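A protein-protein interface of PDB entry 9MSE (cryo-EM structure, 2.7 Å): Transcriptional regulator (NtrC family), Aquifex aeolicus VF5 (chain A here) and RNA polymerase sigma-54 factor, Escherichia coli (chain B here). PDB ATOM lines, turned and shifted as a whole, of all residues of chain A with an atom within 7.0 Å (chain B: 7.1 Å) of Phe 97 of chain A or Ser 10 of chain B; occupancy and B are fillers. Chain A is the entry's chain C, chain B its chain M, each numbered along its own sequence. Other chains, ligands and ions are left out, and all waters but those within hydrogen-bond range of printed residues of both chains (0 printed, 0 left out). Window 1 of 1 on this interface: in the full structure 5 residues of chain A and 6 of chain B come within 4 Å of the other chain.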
ATOM      1  N   ALA A  87     -10.660  15.276   6.180  1.00  0.00           N
ATOM      2  CA  ALA A  87     -10.821  16.676   6.551  1.00  0.00           C
ATOM      3  C   ALA A  87      -9.478  17.353   6.777  1.00  0.00           C
ATOM      4  O   ALA A  87      -9.360  18.568   6.583  1.00  0.00           O
ATOM      5  CB  ALA A  87     -11.694  16.795   7.798  1.00  0.00           C
ATOM      6  N   TYR A  92     -12.561  21.354   4.316  1.00  0.00           N
ATOM      7  CA  TYR A  92     -13.999  21.243   4.130  1.00  0.00           C
ATOM      8  C   TYR A  92     -14.581  22.634   3.929  1.00  0.00           C
ATOM      9  O   TYR A  92     -13.880  23.643   4.020  1.00  0.00           O
ATOM     10  CB  TYR A  92     -14.667  20.536   5.313  1.00  0.00           C
ATOM     11  CG  TYR A  92     -14.428  21.193   6.651  1.00  0.00           C
ATOM     12  CD1 TYR A  92     -15.260  22.200   7.110  1.00  0.00           C
ATOM     13  CD2 TYR A  92     -13.375  20.799   7.458  1.00  0.00           C
ATOM     14  CE1 TYR A  92     -15.045  22.801   8.328  1.00  0.00           C
ATOM     15  CE2 TYR A  92     -13.153  21.392   8.679  1.00  0.00           C
ATOM     16  CZ  TYR A  92     -13.992  22.392   9.109  1.00  0.00           C
ATOM     17  OH  TYR A  92     -13.776  22.989  10.327  1.00  0.00           O
ATOM     18  N   GLU A  93     -15.879  22.674   3.652  1.00  0.00           N
ATOM     19  CA  GLU A  93     -16.612  23.919   3.499  1.00  0.00           C
ATOM     20  C   GLU A  93     -17.739  23.982   4.520  1.00  0.00           C
ATOM     21  O   GLU A  93     -18.128  22.971   5.110  1.00  0.00           O
ATOM     22  CB  GLU A  93     -17.177  24.068   2.085  1.00  0.00           C
ATOM     23  CG  GLU A  93     -16.114  24.180   1.015  1.00  0.00           C
ATOM     24  CD  GLU A  93     -16.662  24.707  -0.291  1.00  0.00           C
ATOM     25  OE1 GLU A  93     -17.858  25.060  -0.332  1.00  0.00           O
ATOM     26  OE2 GLU A  93     -15.896  24.771  -1.277  1.00  0.00           O
ATOM     27  N   LYS A  94     -18.252  25.191   4.732  1.00  0.00           N
ATOM     28  CA  LYS A  94     -19.310  25.396   5.711  1.00  0.00           C
ATOM     29  C   LYS A  94     -20.547  24.591   5.335  1.00  0.00           C
ATOM     30  O   LYS A  94     -20.977  24.595   4.179  1.00  0.00           O
ATOM     31  CB  LYS A  94     -19.652  26.882   5.815  1.00  0.00           C
ATOM     32  CG  LYS A  94     -20.761  27.196   6.803  1.00  0.00           C
ATOM     33  CD  LYS A  94     -20.854  28.688   7.076  1.00  0.00           C
ATOM     34  CE  LYS A  94     -21.147  29.471   5.808  1.00  0.00           C
ATOM     35  NZ  LYS A  94     -22.473  29.118   5.231  1.00  0.00           N
ATOM     36  N   GLY A  95     -21.115  23.900   6.319  1.00  0.00           N
ATOM     37  CA  GLY A  95     -22.267  23.059   6.084  1.00  0.00           C
ATOM     38  C   GLY A  95     -21.959  21.662   5.601  1.00  0.00           C
ATOM     39  O   GLY A  95     -22.889  20.933   5.240  1.00  0.00           O
ATOM     40  N   ALA A  96     -20.685  21.265   5.572  1.00  0.00           N
ATOM     41  CA  ALA A  96     -20.342  19.914   5.138  1.00  0.00           C
ATOM     42  C   ALA A  96     -20.909  18.866   6.085  1.00  0.00           C
ATOM     43  O   ALA A  96     -21.406  17.824   5.644  1.00  0.00           O
ATOM     44  CB  ALA A  96     -18.826  19.769   5.023  1.00  0.00           C
ATOM     45  N   PHE A  97     -20.840  19.122   7.388  1.00  0.00           N
ATOM     46  CA  PHE A  97     -21.365  18.213   8.395  1.00  0.00           C
ATOM     47  C   PHE A  97     -21.822  19.037   9.591  1.00  0.00           C
ATOM     48  O   PHE A  97     -21.731  20.267   9.592  1.00  0.00           O
ATOM     49  CB  PHE A  97     -20.319  17.166   8.792  1.00  0.00           C
ATOM     50  CG  PHE A  97     -18.994  17.750   9.198  1.00  0.00           C
ATOM     51  CD1 PHE A  97     -18.744  18.085  10.516  1.00  0.00           C
ATOM     52  CD2 PHE A  97     -17.996  17.953   8.264  1.00  0.00           C
ATOM     53  CE1 PHE A  97     -17.531  18.621  10.891  1.00  0.00           C
ATOM     54  CE2 PHE A  97     -16.782  18.485   8.635  1.00  0.00           C
ATOM     55  CZ  PHE A  97     -16.550  18.819   9.950  1.00  0.00           C
ATOM     56  N   THR A  98     -22.322  18.351  10.614  1.00  0.00           N
ATOM     57  CA  THR A  98     -22.747  19.025  11.833  1.00  0.00           C
ATOM     58  C   THR A  98     -21.527  19.443  12.641  1.00  0.00           C
ATOM     59  O   THR A  98     -20.659  18.620  12.939  1.00  0.00           O
ATOM     60  CB  THR A  98     -23.646  18.117  12.668  1.00  0.00           C
ATOM     61  OG1 THR A  98     -24.803  17.759  11.904  1.00  0.00           O
ATOM     62  CG2 THR A  98     -24.090  18.830  13.929  1.00  0.00           C
ATOM     63  N   GLY A  99     -21.467  20.720  13.003  1.00  0.00           N
ATOM     64  CA  GLY A  99     -20.317  21.275  13.678  1.00  0.00           C
ATOM     65  C   GLY A  99     -19.365  22.031  12.780  1.00  0.00           C
ATOM     66  O   GLY A  99     -18.440  22.676  13.289  1.00  0.00           O
ATOM     67  N   ALA A 100     -19.560  21.969  11.464  1.00  0.00           N
ATOM     68  CA  ALA A 100     -18.749  22.726  10.513  1.00  0.00           C
ATOM     69  C   ALA A 100     -19.412  24.082  10.313  1.00  0.00           C
ATOM     70  O   ALA A 100     -20.421  24.198   9.615  1.00  0.00           O
ATOM     71  CB  ALA A 100     -18.611  21.971   9.198  1.00  0.00           C
ATOM     72  N   VAL A 101     -18.841  25.114  10.931  1.00  0.00           N
ATOM     73  CA  VAL A 101     -19.414  26.455  10.891  1.00  0.00           C
ATOM     74  C   VAL A 101     -18.608  27.420  10.039  1.00  0.00           C
ATOM     75  O   VAL A 101     -19.060  28.557   9.829  1.00  0.00           O
ATOM     76  CB  VAL A 101     -19.590  27.035  12.310  1.00  0.00           C
ATOM     77  CG1 VAL A 101     -20.634  26.244  13.077  1.00  0.00           C
ATOM     78  CG2 VAL A 101     -18.266  27.022  13.049  1.00  0.00           C
ATOM     79  N   LEU A 144     -14.312  18.751   1.191  1.00  0.00           N
ATOM     80  CA  LEU A 144     -15.504  18.094   1.712  1.00  0.00           C
ATOM     81  C   LEU A 144     -16.702  19.029   1.644  1.00  0.00           C
ATOM     82  O   LEU A 144     -16.758  20.030   2.363  1.00  0.00           O
ATOM     83  CB  LEU A 144     -15.282  17.626   3.151  1.00  0.00           C
ATOM     84  CG  LEU A 144     -14.813  16.187   3.359  1.00  0.00           C
ATOM     85  CD1 LEU A 144     -13.467  15.955   2.706  1.00  0.00           C
ATOM     86  CD2 LEU A 144     -14.754  15.866   4.840  1.00  0.00           C
ATOM     87  N   ARG B   8     -15.616  11.847  15.068  1.00  0.00           N
ATOM     88  CA  ARG B   8     -16.054  11.584  13.704  1.00  0.00           C
ATOM     89  C   ARG B   8     -16.913  12.737  13.211  1.00  0.00           C
ATOM     90  O   ARG B   8     -17.380  13.573  13.987  1.00  0.00           O
ATOM     91  CB  ARG B   8     -16.815  10.260  13.614  1.00  0.00           C
ATOM     92  CG  ARG B   8     -17.959  10.134  14.599  1.00  0.00           C
ATOM     93  CD  ARG B   8     -18.673   8.800  14.456  1.00  0.00           C
ATOM     94  NE  ARG B   8     -17.792   7.669  14.719  1.00  0.00           N
ATOM     95  CZ  ARG B   8     -17.209   6.935  13.780  1.00  0.00           C
ATOM     96  NH1 ARG B   8     -17.399   7.180  12.494  1.00  0.00           N
ATOM     97  NH2 ARG B   8     -16.417   5.930  14.140  1.00  0.00           N
ATOM     98  N   LEU B   9     -17.113  12.765  11.895  1.00  0.00           N
ATOM     99  CA  LEU B   9     -17.915  13.782  11.227  1.00  0.00           C
ATOM    100  C   LEU B   9     -19.266  13.167  10.879  1.00  0.00           C
ATOM    101  O   LEU B   9     -19.351  12.300  10.004  1.00  0.00           O
ATOM    102  CB  LEU B   9     -17.207  14.287   9.973  1.00  0.00           C
ATOM    103  CG  LEU B   9     -15.687  14.438  10.041  1.00  0.00           C
ATOM    104  CD1 LEU B   9     -15.123  14.694   8.657  1.00  0.00           C
ATOM    105  CD2 LEU B   9     -15.295  15.553  10.986  1.00  0.00           C
ATOM    106  N   SER B  10     -20.317  13.618  11.554  1.00  0.00           N
ATOM    107  CA  SER B  10     -21.647  13.052  11.397  1.00  0.00           C
ATOM    108  C   SER B  10     -22.653  14.144  11.060  1.00  0.00           C
ATOM    109  O   SER B  10     -22.366  15.340  11.145  1.00  0.00           O
ATOM    110  CB  SER B  10     -22.085  12.312  12.668  1.00  0.00           C
ATOM    111  OG  SER B  10     -21.241  11.207  12.938  1.00  0.00           O
ATOM    112  N   GLN B  11     -23.846  13.709  10.668  1.00  0.00           N
ATOM    113  CA  GLN B  11     -24.980  14.591  10.409  1.00  0.00           C
ATOM    114  C   GLN B  11     -26.089  14.211  11.379  1.00  0.00           C
ATOM    115  O   GLN B  11     -26.638  13.108  11.299  1.00  0.00           O
ATOM    116  CB  GLN B  11     -25.445  14.472   8.963  1.00  0.00           C
ATOM    117  CG  GLN B  11     -24.367  14.796   7.957  1.00  0.00           C
ATOM    118  CD  GLN B  11     -24.841  14.631   6.538  1.00  0.00           C
ATOM    119  OE1 GLN B  11     -24.251  15.179   5.610  1.00  0.00           O
ATOM    120  NE2 GLN B  11     -25.911  13.870   6.357  1.00  0.00           N
ATOM    121  N   GLN B  12     -26.423  15.123  12.289  1.00  0.00           N
ATOM    122  CA  GLN B  12     -27.306  14.805  13.398  1.00  0.00           C
ATOM    123  C   GLN B  12     -28.341  15.903  13.580  1.00  0.00           C
ATOM    124  O   GLN B  12     -28.127  17.053  13.191  1.00  0.00           O
ATOM    125  CB  GLN B  12     -26.522  14.626  14.703  1.00  0.00           C
ATOM    126  CG  GLN B  12     -25.512  13.496  14.679  1.00  0.00           C
ATOM    127  CD  GLN B  12     -24.516  13.593  15.812  1.00  0.00           C
ATOM    128  OE1 GLN B  12     -24.515  14.562  16.570  1.00  0.00           O
ATOM    129  NE2 GLN B  12     -23.656  12.589  15.933  1.00  0.00           N
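O of Ser 10 of chain B lies within hydrogen-bond range of N of Thr 98 of chain A (3.1 Å).
The side-chain hydroxyl (OG1) of Thr 98 of chain A is in hydrogen-bond range of the backbone NH (N) of Gln 12 of chain B (3.1 Å).
Among the printed residues, merely in contact across the chains: Thr 98 of chain A with Gln 11 of chain B (3.5 Å), Phe 97 of chain A with Ser 10 of chain B (3.6 Å), Phe 97 of chain A with Leu 9 of chain B (3.6 Å) and Ala 96 of chain A with Gln 11 of chain B (3.9 Å).
Printed residues of chain B within 4 Å of Ala 96 of chain A: Gln 11.
Phe 97 of chain A touches two residues of chain B.
Printed residues of chain B within 4 Å of Thr 98 of chain A: Ser 10, Gln 11 and Gln 12.
Printed residues of chain A within 4 Å of Leu 9 of chain B: Phe 97.
Of the printed residues of chain A, Gln 11 of chain B touches Ala 96 and Thr 98.
Of the printed residues of chain A, Gln 12 of chain B touches Thr 98.
The nearest residue of chain B that does not touch Phe 97 of chain A is Gln 11 of chain B (4.6 Å).
The nearest residue of chain A that does not touch Ser 10 of chain B is Gly 99 of chain A (5.8 Å).
The nearest printed residue of chain B that does not touch Ala 96 of chain A is Ser 10 of chain B (6.1 Å).
Of the 5 printed residues of chain B, 4 touch a printed residue of chain A.
Printed residues of chain B that touch a printed residue of chain A: Leu 9, Ser 10, Gln 11 and Gln 12.
Along chain B the printed residues that touch a printed residue of chain A span positions 9 to 12.
Among the printed residues, no Asp or Glu carboxylate lies within 4 Å of a Lys or Arg side-chain nitrogen of the other chain.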
